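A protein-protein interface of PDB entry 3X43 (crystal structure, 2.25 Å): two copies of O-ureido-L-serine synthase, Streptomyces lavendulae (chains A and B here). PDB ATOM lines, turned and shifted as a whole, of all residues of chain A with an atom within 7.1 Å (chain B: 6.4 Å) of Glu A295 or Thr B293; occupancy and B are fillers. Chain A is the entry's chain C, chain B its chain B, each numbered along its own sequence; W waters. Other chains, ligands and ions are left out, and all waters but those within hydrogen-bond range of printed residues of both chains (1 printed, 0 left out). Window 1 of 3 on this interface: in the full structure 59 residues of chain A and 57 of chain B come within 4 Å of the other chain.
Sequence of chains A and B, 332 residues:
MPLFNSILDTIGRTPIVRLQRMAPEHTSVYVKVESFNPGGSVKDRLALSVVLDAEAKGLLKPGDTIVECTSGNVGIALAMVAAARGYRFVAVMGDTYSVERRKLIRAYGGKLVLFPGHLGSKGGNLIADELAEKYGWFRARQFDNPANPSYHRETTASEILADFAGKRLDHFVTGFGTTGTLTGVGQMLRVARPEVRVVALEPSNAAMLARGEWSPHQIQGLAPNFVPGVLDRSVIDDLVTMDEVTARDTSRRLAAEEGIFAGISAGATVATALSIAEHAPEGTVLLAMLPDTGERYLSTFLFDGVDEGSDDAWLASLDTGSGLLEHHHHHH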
ATOM      1  N   PRO A  38      13.374 -23.779 -11.032  1.00  0.00           N
ATOM      2  CA  PRO A  38      14.761 -24.029 -10.604  1.00  0.00           C
ATOM      3  C   PRO A  38      15.245 -25.456 -10.883  1.00  0.00           C
ATOM      4  O   PRO A  38      16.406 -25.675 -11.231  1.00  0.00           O
ATOM      5  CB  PRO A  38      14.748 -23.724  -9.107  1.00  0.00           C
ATOM      6  CG  PRO A  38      13.267 -23.684  -8.715  1.00  0.00           C
ATOM      7  CD  PRO A  38      12.548 -23.218  -9.948  1.00  0.00           C
ATOM      8  N   GLU A 100      24.018 -39.804 -16.125  1.00  0.00           N
ATOM      9  CA  GLU A 100      23.820 -38.368 -15.978  1.00  0.00           C
ATOM     10  C   GLU A 100      22.656 -38.130 -15.035  1.00  0.00           C
ATOM     11  O   GLU A 100      22.688 -37.224 -14.202  1.00  0.00           O
ATOM     12  CB  GLU A 100      23.539 -37.718 -17.334  1.00  0.00           C
ATOM     13  CG  GLU A 100      22.947 -38.650 -18.371  1.00  0.00           C
ATOM     14  CD  GLU A 100      21.513 -38.291 -18.727  1.00  0.00           C
ATOM     15  OE1 GLU A 100      20.929 -38.954 -19.619  1.00  0.00           O
ATOM     16  OE2 GLU A 100      20.970 -37.343 -18.115  1.00  0.00           O
ATOM     17  N   TYR A 108      22.373 -32.748  -5.853  1.00  0.00           N
ATOM     18  CA  TYR A 108      21.509 -32.148  -4.838  1.00  0.00           C
ATOM     19  C   TYR A 108      21.599 -32.863  -3.490  1.00  0.00           C
ATOM     20  O   TYR A 108      20.748 -32.668  -2.627  1.00  0.00           O
ATOM     21  CB  TYR A 108      20.049 -32.141  -5.316  1.00  0.00           C
ATOM     22  CG  TYR A 108      19.731 -31.096  -6.373  1.00  0.00           C
ATOM     23  CD1 TYR A 108      19.717 -29.733  -6.058  1.00  0.00           C
ATOM     24  CD2 TYR A 108      19.436 -31.475  -7.686  1.00  0.00           C
ATOM     25  CE1 TYR A 108      19.411 -28.770  -7.037  1.00  0.00           C
ATOM     26  CE2 TYR A 108      19.128 -30.517  -8.665  1.00  0.00           C
ATOM     27  CZ  TYR A 108      19.117 -29.175  -8.331  1.00  0.00           C
ATOM     28  OH  TYR A 108      18.796 -28.244  -9.283  1.00  0.00           O
ATOM     29  N   PHE A 261      14.901 -24.567 -26.277  1.00  0.00           N
ATOM     30  CA  PHE A 261      15.462 -25.900 -26.093  1.00  0.00           C
ATOM     31  C   PHE A 261      14.702 -26.659 -25.005  1.00  0.00           C
ATOM     32  O   PHE A 261      14.921 -26.434 -23.819  1.00  0.00           O
ATOM     33  CB  PHE A 261      16.942 -25.757 -25.713  1.00  0.00           C
ATOM     34  CG  PHE A 261      17.716 -27.049 -25.737  1.00  0.00           C
ATOM     35  CD1 PHE A 261      17.352 -28.087 -26.596  1.00  0.00           C
ATOM     36  CD2 PHE A 261      18.815 -27.223 -24.898  1.00  0.00           C
ATOM     37  CE1 PHE A 261      18.072 -29.282 -26.617  1.00  0.00           C
ATOM     38  CE2 PHE A 261      19.542 -28.413 -24.909  1.00  0.00           C
ATOM     39  CZ  PHE A 261      19.170 -29.444 -25.770  1.00  0.00           C
ATOM     40  N   ALA A 262      13.813 -27.561 -25.419  1.00  0.00           N
ATOM     41  CA  ALA A 262      13.010 -28.345 -24.484  1.00  0.00           C
ATOM     42  C   ALA A 262      13.100 -29.840 -24.775  1.00  0.00           C
ATOM     43  O   ALA A 262      13.569 -30.244 -25.833  1.00  0.00           O
ATOM     44  CB  ALA A 262      11.553 -27.892 -24.545  1.00  0.00           C
ATOM     45  N   GLY A 263      12.625 -30.653 -23.837  1.00  0.00           N
ATOM     46  CA  GLY A 263      12.669 -32.094 -24.004  1.00  0.00           C
ATOM     47  C   GLY A 263      11.785 -32.670 -25.095  1.00  0.00           C
ATOM     48  O   GLY A 263      11.078 -31.949 -25.803  1.00  0.00           O
ATOM     49  N   ASP A 292       9.985 -29.858 -19.812  1.00  0.00           N
ATOM     50  CA  ASP A 292      11.328 -29.615 -19.313  1.00  0.00           C
ATOM     51  C   ASP A 292      12.347 -29.112 -20.302  1.00  0.00           C
ATOM     52  O   ASP A 292      12.061 -28.931 -21.492  1.00  0.00           O
ATOM     53  CB  ASP A 292      11.875 -30.877 -18.622  1.00  0.00           C
ATOM     54  CG  ASP A 292      12.062 -32.048 -19.578  1.00  0.00           C
ATOM     55  OD1 ASP A 292      11.913 -31.866 -20.808  1.00  0.00           O
ATOM     56  OD2 ASP A 292      12.365 -33.164 -19.090  1.00  0.00           O
ATOM     57  N   THR A 293      13.543 -28.888 -19.766  1.00  0.00           N
ATOM     58  CA  THR A 293      14.707 -28.410 -20.504  1.00  0.00           C
ATOM     59  C   THR A 293      15.339 -29.527 -21.333  1.00  0.00           C
ATOM     60  O   THR A 293      15.462 -30.661 -20.871  1.00  0.00           O
ATOM     61  CB  THR A 293      15.781 -27.899 -19.538  1.00  0.00           C
ATOM     62  OG1 THR A 293      16.936 -27.492 -20.276  1.00  0.00           O
ATOM     63  CG2 THR A 293      16.182 -29.005 -18.572  1.00  0.00           C
ATOM     64  N   GLY A 294      15.750 -29.199 -22.553  1.00  0.00           N
ATOM     65  CA  GLY A 294      16.374 -30.197 -23.397  1.00  0.00           C
ATOM     66  C   GLY A 294      17.805 -30.505 -22.980  1.00  0.00           C
ATOM     67  O   GLY A 294      18.365 -31.523 -23.385  1.00  0.00           O
ATOM     68  N   GLU A 295      18.394 -29.639 -22.157  1.00  0.00           N
ATOM     69  CA  GLU A 295      19.772 -29.833 -21.715  1.00  0.00           C
ATOM     70  C   GLU A 295      20.052 -31.184 -21.050  1.00  0.00           C
ATOM     71  O   GLU A 295      21.211 -31.590 -20.936  1.00  0.00           O
ATOM     72  CB  GLU A 295      20.207 -28.695 -20.781  1.00  0.00           C
ATOM     73  CG  GLU A 295      21.625 -28.197 -21.062  1.00  0.00           C
ATOM     74  CD  GLU A 295      22.077 -27.096 -20.111  1.00  0.00           C
ATOM     75  OE1 GLU A 295      23.238 -26.644 -20.234  1.00  0.00           O
ATOM     76  OE2 GLU A 295      21.277 -26.678 -19.241  1.00  0.00           O
ATOM     77  N   ARG A 296      19.014 -31.882 -20.600  1.00  0.00           N
ATOM     78  CA  ARG A 296      19.251 -33.182 -19.990  1.00  0.00           C
ATOM     79  C   ARG A 296      18.812 -34.298 -20.917  1.00  0.00           C
ATOM     80  O   ARG A 296      18.385 -35.358 -20.471  1.00  0.00           O
ATOM     81  CB  ARG A 296      18.552 -33.316 -18.627  1.00  0.00           C
ATOM     82  CG  ARG A 296      17.182 -32.701 -18.504  1.00  0.00           C
ATOM     83  CD  ARG A 296      16.669 -32.851 -17.064  1.00  0.00           C
ATOM     84  NE  ARG A 296      17.274 -31.885 -16.149  1.00  0.00           N
ATOM     85  CZ  ARG A 296      16.621 -31.273 -15.163  1.00  0.00           C
ATOM     86  NH1 ARG A 296      15.335 -31.522 -14.953  1.00  0.00           N
ATOM     87  NH2 ARG A 296      17.253 -30.406 -14.381  1.00  0.00           N
ATOM     88  N   TYR A 297      18.939 -34.053 -22.215  1.00  0.00           N
ATOM     89  CA  TYR A 297      18.566 -35.041 -23.214  1.00  0.00           C
ATOM     90  C   TYR A 297      19.680 -35.271 -24.229  1.00  0.00           C
ATOM     91  O   TYR A 297      19.430 -35.792 -25.317  1.00  0.00           O
ATOM     92  CB  TYR A 297      17.292 -34.599 -23.932  1.00  0.00           C
ATOM     93  CG  TYR A 297      16.054 -34.751 -23.082  1.00  0.00           C
ATOM     94  CD1 TYR A 297      15.225 -35.863 -23.218  1.00  0.00           C
ATOM     95  CD2 TYR A 297      15.727 -33.791 -22.121  1.00  0.00           C
ATOM     96  CE1 TYR A 297      14.099 -36.013 -22.415  1.00  0.00           C
ATOM     97  CE2 TYR A 297      14.609 -33.937 -21.319  1.00  0.00           C
ATOM     98  CZ  TYR A 297      13.799 -35.047 -21.470  1.00  0.00           C
ATOM     99  OH  TYR A 297      12.687 -35.187 -20.674  1.00  0.00           O
ATOM    100  N   LEU A 298      20.907 -34.891 -23.868  1.00  0.00           N
ATOM    101  CA  LEU A 298      22.061 -35.059 -24.754  1.00  0.00           C
ATOM    102  C   LEU A 298      22.454 -36.528 -24.905  1.00  0.00           C
ATOM    103  O   LEU A 298      22.954 -36.938 -25.951  1.00  0.00           O
ATOM    104  CB  LEU A 298      23.262 -34.261 -24.233  1.00  0.00           C
ATOM    105  CG  LEU A 298      23.020 -32.842 -23.710  1.00  0.00           C
ATOM    106  CD1 LEU A 298      24.065 -32.520 -22.646  1.00  0.00           C
ATOM    107  CD2 LEU A 298      23.090 -31.836 -24.853  1.00  0.00           C
ATOM    108  N   SER A 299      22.225 -37.313 -23.857  1.00  0.00           N
ATOM    109  CA  SER A 299      22.538 -38.738 -23.867  1.00  0.00           C
ATOM    110  C   SER A 299      21.287 -39.530 -24.245  1.00  0.00           C
ATOM    111  O   SER A 299      21.124 -40.686 -23.854  1.00  0.00           O
ATOM    112  CB  SER A 299      23.033 -39.182 -22.486  1.00  0.00           C
ATOM    113  OG  SER A 299      24.122 -38.383 -22.049  1.00  0.00           O
ATOM    114  N   LEU A 302      17.689 -37.824 -28.692  1.00  0.00           N
ATOM    115  CA  LEU A 302      17.341 -36.462 -29.073  1.00  0.00           C
ATOM    116  C   LEU A 302      18.486 -35.970 -29.943  1.00  0.00           C
ATOM    117  O   LEU A 302      18.339 -35.030 -30.719  1.00  0.00           O
ATOM    118  CB  LEU A 302      17.219 -35.571 -27.833  1.00  0.00           C
ATOM    119  CG  LEU A 302      16.270 -34.365 -27.869  1.00  0.00           C
ATOM    120  CD1 LEU A 302      16.828 -33.277 -26.972  1.00  0.00           C
ATOM    121  CD2 LEU A 302      16.099 -33.841 -29.289  1.00  0.00           C
ATOM    122  N   PHE A 303      19.633 -36.625 -29.795  1.00  0.00           N
ATOM    123  CA  PHE A 303      20.835 -36.297 -30.552  1.00  0.00           C
ATOM    124  C   PHE A 303      21.368 -37.559 -31.236  1.00  0.00           C
ATOM    125  O   PHE A 303      22.570 -37.829 -31.215  1.00  0.00           O
ATOM    126  CB  PHE A 303      21.909 -35.726 -29.618  1.00  0.00           C
ATOM    127  CG  PHE A 303      21.548 -34.397 -29.011  1.00  0.00           C
ATOM    128  CD1 PHE A 303      20.928 -34.331 -27.766  1.00  0.00           C
ATOM    129  CD2 PHE A 303      21.844 -33.210 -29.675  1.00  0.00           C
ATOM    130  CE1 PHE A 303      20.611 -33.101 -27.189  1.00  0.00           C
ATOM    131  CE2 PHE A 303      21.531 -31.976 -29.106  1.00  0.00           C
ATOM    132  CZ  PHE A 303      20.913 -31.923 -27.861  1.00  0.00           C
ATOM    133  N   GLU B  34      21.570 -16.502 -12.119  1.00  0.00           N
ATOM    134  CA  GLU B  34      21.489 -16.185 -13.539  1.00  0.00           C
ATOM    135  C   GLU B  34      21.128 -17.377 -14.413  1.00  0.00           C
ATOM    136  O   GLU B  34      21.030 -17.251 -15.634  1.00  0.00           O
ATOM    137  CB  GLU B  34      22.799 -15.568 -14.018  1.00  0.00           C
ATOM    138  CG  GLU B  34      23.023 -14.148 -13.485  1.00  0.00           C
ATOM    139  CD  GLU B  34      22.073 -13.123 -14.106  1.00  0.00           C
ATOM    140  OE1 GLU B  34      21.499 -12.308 -13.357  1.00  0.00           O
ATOM    141  OE2 GLU B  34      21.899 -13.132 -15.341  1.00  0.00           O
ATOM    142  N   SER B  35      20.917 -18.530 -13.791  1.00  0.00           N
ATOM    143  CA  SER B  35      20.545 -19.732 -14.525  1.00  0.00           C
ATOM    144  C   SER B  35      19.068 -19.652 -14.890  1.00  0.00           C
ATOM    145  O   SER B  35      18.560 -20.460 -15.677  1.00  0.00           O
ATOM    146  CB  SER B  35      20.797 -20.988 -13.675  1.00  0.00           C
ATOM    147  OG  SER B  35      20.005 -20.989 -12.497  1.00  0.00           O
ATOM    148  N   GLY B  39      18.792 -18.983 -21.423  1.00  0.00           N
ATOM    149  CA  GLY B  39      20.043 -19.555 -21.890  1.00  0.00           C
ATOM    150  C   GLY B  39      20.820 -20.282 -20.804  1.00  0.00           C
ATOM    151  O   GLY B  39      21.896 -20.827 -21.058  1.00  0.00           O
ATOM    152  N   GLY B  40      20.281 -20.277 -19.588  1.00  0.00           N
ATOM    153  CA  GLY B  40      20.928 -20.963 -18.482  1.00  0.00           C
ATOM    154  C   GLY B  40      22.166 -20.282 -17.951  1.00  0.00           C
ATOM    155  O   GLY B  40      22.938 -20.875 -17.189  1.00  0.00           O
ATOM    156  N   SER B  41      22.361 -19.032 -18.338  1.00  0.00           N
ATOM    157  CA  SER B  41      23.523 -18.290 -17.884  1.00  0.00           C
ATOM    158  C   SER B  41      23.374 -16.790 -18.074  1.00  0.00           C
ATOM    159  O   SER B  41      22.505 -16.312 -18.817  1.00  0.00           O
ATOM    160  CB  SER B  41      24.774 -18.778 -18.618  1.00  0.00           C
ATOM    161  OG  SER B  41      25.362 -17.748 -19.388  1.00  0.00           O
ATOM    162  N   ILE B  76      26.577 -20.497 -26.508  1.00  0.00           N
ATOM    163  CA  ILE B  76      25.227 -21.015 -26.291  1.00  0.00           C
ATOM    164  C   ILE B  76      24.172 -19.899 -26.314  1.00  0.00           C
ATOM    165  O   ILE B  76      23.082 -20.074 -26.854  1.00  0.00           O
ATOM    166  CB  ILE B  76      25.147 -21.768 -24.945  1.00  0.00           C
ATOM    167  CG1 ILE B  76      26.089 -22.977 -24.974  1.00  0.00           C
ATOM    168  CG2 ILE B  76      23.714 -22.205 -24.663  1.00  0.00           C
ATOM    169  CD1 ILE B  76      26.156 -23.734 -23.663  1.00  0.00           C
ATOM    170  N   LEU B 104      25.158 -28.819 -27.463  1.00  0.00           N
ATOM    171  CA  LEU B 104      24.353 -27.689 -27.026  1.00  0.00           C
ATOM    172  C   LEU B 104      24.245 -26.646 -28.128  1.00  0.00           C
ATOM    173  O   LEU B 104      23.157 -26.148 -28.416  1.00  0.00           O
ATOM    174  CB  LEU B 104      24.970 -27.051 -25.783  1.00  0.00           C
ATOM    175  CG  LEU B 104      24.045 -26.713 -24.608  1.00  0.00           C
ATOM    176  CD1 LEU B 104      22.586 -26.958 -24.975  1.00  0.00           C
ATOM    177  CD2 LEU B 104      24.448 -27.556 -23.404  1.00  0.00           C
ATOM    178  N   PHE B 261      21.556 -25.355  -7.726  1.00  0.00           N
ATOM    179  CA  PHE B 261      22.555 -26.015  -8.554  1.00  0.00           C
ATOM    180  C   PHE B 261      23.185 -25.090  -9.584  1.00  0.00           C
ATOM    181  O   PHE B 261      22.625 -24.864 -10.658  1.00  0.00           O
ATOM    182  CB  PHE B 261      21.914 -27.225  -9.251  1.00  0.00           C
ATOM    183  CG  PHE B 261      22.897 -28.128  -9.939  1.00  0.00           C
ATOM    184  CD1 PHE B 261      24.163 -28.338  -9.408  1.00  0.00           C
ATOM    185  CD2 PHE B 261      22.555 -28.768 -11.123  1.00  0.00           C
ATOM    186  CE1 PHE B 261      25.074 -29.174 -10.050  1.00  0.00           C
ATOM    187  CE2 PHE B 261      23.464 -29.607 -11.772  1.00  0.00           C
ATOM    188  CZ  PHE B 261      24.718 -29.808 -11.235  1.00  0.00           C
ATOM    189  N   ALA B 262      24.366 -24.578  -9.258  1.00  0.00           N
ATOM    190  CA  ALA B 262      25.079 -23.664 -10.132  1.00  0.00           C
ATOM    191  C   ALA B 262      26.446 -24.229 -10.482  1.00  0.00           C
ATOM    192  O   ALA B 262      26.798 -25.317 -10.033  1.00  0.00           O
ATOM    193  CB  ALA B 262      25.223 -22.322  -9.457  1.00  0.00           C
ATOM    194  N   GLY B 263      27.209 -23.479 -11.278  1.00  0.00           N
ATOM    195  CA  GLY B 263      28.529 -23.917 -11.710  1.00  0.00           C
ATOM    196  C   GLY B 263      29.697 -23.532 -10.821  1.00  0.00           C
ATOM    197  O   GLY B 263      29.496 -23.118  -9.681  1.00  0.00           O
ATOM    198  N   LEU B 290      25.627 -15.768  -9.185  1.00  0.00           N
ATOM    199  CA  LEU B 290      25.628 -17.176  -9.586  1.00  0.00           C
ATOM    200  C   LEU B 290      25.437 -17.120 -11.114  1.00  0.00           C
ATOM    201  O   LEU B 290      24.317 -17.155 -11.614  1.00  0.00           O
ATOM    202  CB  LEU B 290      24.445 -17.894  -8.934  1.00  0.00           C
ATOM    203  CG  LEU B 290      24.660 -18.612  -7.603  1.00  0.00           C
ATOM    204  CD1 LEU B 290      25.461 -17.746  -6.653  1.00  0.00           C
ATOM    205  CD2 LEU B 290      23.312 -18.964  -7.013  1.00  0.00           C
ATOM    206  N   PRO B 291      26.539 -17.084 -11.867  1.00  0.00           N
ATOM    207  CA  PRO B 291      26.467 -16.999 -13.331  1.00  0.00           C
ATOM    208  C   PRO B 291      25.752 -18.040 -14.182  1.00  0.00           C
ATOM    209  O   PRO B 291      25.228 -17.698 -15.240  1.00  0.00           O
ATOM    210  CB  PRO B 291      27.935 -16.820 -13.749  1.00  0.00           C
ATOM    211  CG  PRO B 291      28.654 -16.398 -12.470  1.00  0.00           C
ATOM    212  CD  PRO B 291      27.933 -17.142 -11.395  1.00  0.00           C
ATOM    213  N   ASP B 292      25.713 -19.297 -13.765  1.00  0.00           N
ATOM    214  CA  ASP B 292      25.056 -20.281 -14.610  1.00  0.00           C
ATOM    215  C   ASP B 292      24.626 -21.553 -13.910  1.00  0.00           C
ATOM    216  O   ASP B 292      24.908 -21.744 -12.722  1.00  0.00           O
ATOM    217  CB  ASP B 292      25.952 -20.621 -15.814  1.00  0.00           C
ATOM    218  CG  ASP B 292      27.223 -21.403 -15.431  1.00  0.00           C
ATOM    219  OD1 ASP B 292      27.483 -21.638 -14.230  1.00  0.00           O
ATOM    220  OD2 ASP B 292      27.971 -21.788 -16.359  1.00  0.00           O
ATOM    221  N   THR B 293      23.926 -22.409 -14.653  1.00  0.00           N
ATOM    222  CA  THR B 293      23.441 -23.676 -14.116  1.00  0.00           C
ATOM    223  C   THR B 293      24.546 -24.724 -14.071  1.00  0.00           C
ATOM    224  O   THR B 293      25.356 -24.828 -14.995  1.00  0.00           O
ATOM    225  CB  THR B 293      22.283 -24.253 -14.952  1.00  0.00           C
ATOM    226  OG1 THR B 293      22.004 -25.586 -14.513  1.00  0.00           O
ATOM    227  CG2 THR B 293      22.643 -24.290 -16.430  1.00  0.00           C
ATOM    228  N   GLY B 294      24.569 -25.501 -12.989  1.00  0.00           N
ATOM    229  CA  GLY B 294      25.573 -26.538 -12.850  1.00  0.00           C
ATOM    230  C   GLY B 294      25.303 -27.714 -13.771  1.00  0.00           C
ATOM    231  O   GLY B 294      26.132 -28.614 -13.889  1.00  0.00           O
ATOM    232  N   GLU B 295      24.153 -27.707 -14.440  1.00  0.00           N
ATOM    233  CA  GLU B 295      23.793 -28.809 -15.320  1.00  0.00           C
ATOM    234  C   GLU B 295      24.714 -29.038 -16.517  1.00  0.00           C
ATOM    235  O   GLU B 295      24.760 -30.140 -17.048  1.00  0.00           O
ATOM    236  CB  GLU B 295      22.353 -28.655 -15.813  1.00  0.00           C
ATOM    237  CG  GLU B 295      21.804 -29.924 -16.450  1.00  0.00           C
ATOM    238  CD  GLU B 295      20.354 -30.199 -16.093  1.00  0.00           C
ATOM    239  OE1 GLU B 295      19.753 -31.114 -16.696  1.00  0.00           O
ATOM    240  OE2 GLU B 295      19.812 -29.503 -15.210  1.00  0.00           O
ATOM    241  N   ARG B 296      25.440 -28.020 -16.962  1.00  0.00           N
ATOM    242  CA  ARG B 296      26.335 -28.235 -18.096  1.00  0.00           C
ATOM    243  C   ARG B 296      27.759 -28.553 -17.649  1.00  0.00           C
ATOM    244  O   ARG B 296      28.695 -28.459 -18.441  1.00  0.00           O
ATOM    245  CB  ARG B 296      26.337 -27.025 -19.048  1.00  0.00           C
ATOM    246  CG  ARG B 296      26.563 -25.666 -18.415  1.00  0.00           C
ATOM    247  CD  ARG B 296      26.240 -24.547 -19.417  1.00  0.00           C
ATOM    248  NE  ARG B 296      24.907 -24.705 -20.000  1.00  0.00           N
ATOM    249  CZ  ARG B 296      24.094 -23.699 -20.318  1.00  0.00           C
ATOM    250  NH1 ARG B 296      24.463 -22.443 -20.115  1.00  0.00           N
ATOM    251  NH2 ARG B 296      22.896 -23.950 -20.832  1.00  0.00           N
ATOM    252  N   TYR B 297      27.905 -28.957 -16.386  1.00  0.00           N
ATOM    253  CA  TYR B 297      29.210 -29.281 -15.812  1.00  0.00           C
ATOM    254  C   TYR B 297      29.387 -30.753 -15.450  1.00  0.00           C
ATOM    255  O   TYR B 297      30.426 -31.144 -14.917  1.00  0.00           O
ATOM    256  CB  TYR B 297      29.446 -28.438 -14.559  1.00  0.00           C
ATOM    257  CG  TYR B 297      29.659 -26.977 -14.855  1.00  0.00           C
ATOM    258  CD1 TYR B 297      30.925 -26.497 -15.191  1.00  0.00           C
ATOM    259  CD2 TYR B 297      28.590 -26.082 -14.841  1.00  0.00           C
ATOM    260  CE1 TYR B 297      31.123 -25.158 -15.510  1.00  0.00           C
ATOM    261  CE2 TYR B 297      28.782 -24.740 -15.160  1.00  0.00           C
ATOM    262  CZ  TYR B 297      30.048 -24.285 -15.493  1.00  0.00           C
ATOM    263  OH  TYR B 297      30.246 -22.955 -15.795  1.00  0.00           O
HETATM  264  O   HOH W   1      18.715 -25.632  -8.173  1.00  0.00           O
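Glu A295 touches Thr B293, but with the chains exchanged Thr A293 does not touch Glu B295 (4.6 Å).
Glu A295 touches Arg B296, and with the chains exchanged Arg A296 touches Glu B295.
Of the 6 pairs that touch across the chains among the printed residues, 2 have their exchanged pair printed and touching as well.
The side-chain carboxylate (OE1) of Glu B295 is in salt-bridge range of the guanidinium group (NE) of Arg A296.
The guanidinium group (NE) of Arg B296 is in salt-bridge range of the side-chain carboxylate (OE1) of Glu A295, at 2.6 Å.
Gly A294 touches none of the printed residues of chain B.
Of chain B, only Leu B104, Thr B293 and Arg B296 come within 4 Å of Glu A295.
Printed residues of chain A within 4 Å of Leu B104: Phe A261 and Glu A295.
Of chain A, only Glu A295 comes within 4 Å of Thr B293.
Printed residues of chain A within 4 Å of Arg B296: Glu A295 (2.6 Å).
The nearest residue of chain B that does not touch Glu A295 is Glu B295 (4.1 Å).
The nearest residue of chain A that does not touch Thr B293 is Pro A38 (6.5 Å).
The nearest printed residue of chain A that does not touch Phe B261 is Pro A38 (6.1 Å).
Of the 16 printed residues of chain A, 4 touch a printed residue of chain B.
Hydrophobic or aromatic side chains of chain A within 4 Å of the printed part of chain B: Tyr A108 and Phe A261.
Of the 18 printed residues of chain B, 5 touch a printed residue of chain A.
Hydrophobic or aromatic side chains of chain B within 4 Å of the printed part of chain A: Leu B104 and Phe B261.
Among the printed residues, merely in contact across the chains: Tyr A108 with Phe B261 (3.3 Å), Phe A261 with Leu B104 (3.4 Å), Glu A295 with Leu B104 (3.5 Å) and Glu A295 with Thr B293 (3.9 Å).
N of Glu B295 is in hydrogen-bond range of OG1 of Thr B293.
O of Gly B39 sits at hydrogen-bond distance from NH1 of Arg B296, at 3.2 Å.
The backbone NH of Gly A294 lies within hydrogen-bond range of the backbone carbonyl oxygen of Phe A261 (3.2 Å).
O of Gly B40 lies within hydrogen-bond range of N of Thr B293.
The backbone NH (N) of Gly B294 is in hydrogen-bond range of the backbone carbonyl oxygen (O) of Phe B261 (3.1 Å).
N of Glu A295 lies close to OG1 of Thr A293 (3.2 Å).
Water W1 bridges the side-chain hydroxyl of Tyr A108 (2.8 Å) and the backbone NH of Phe B261 (2.9 Å).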
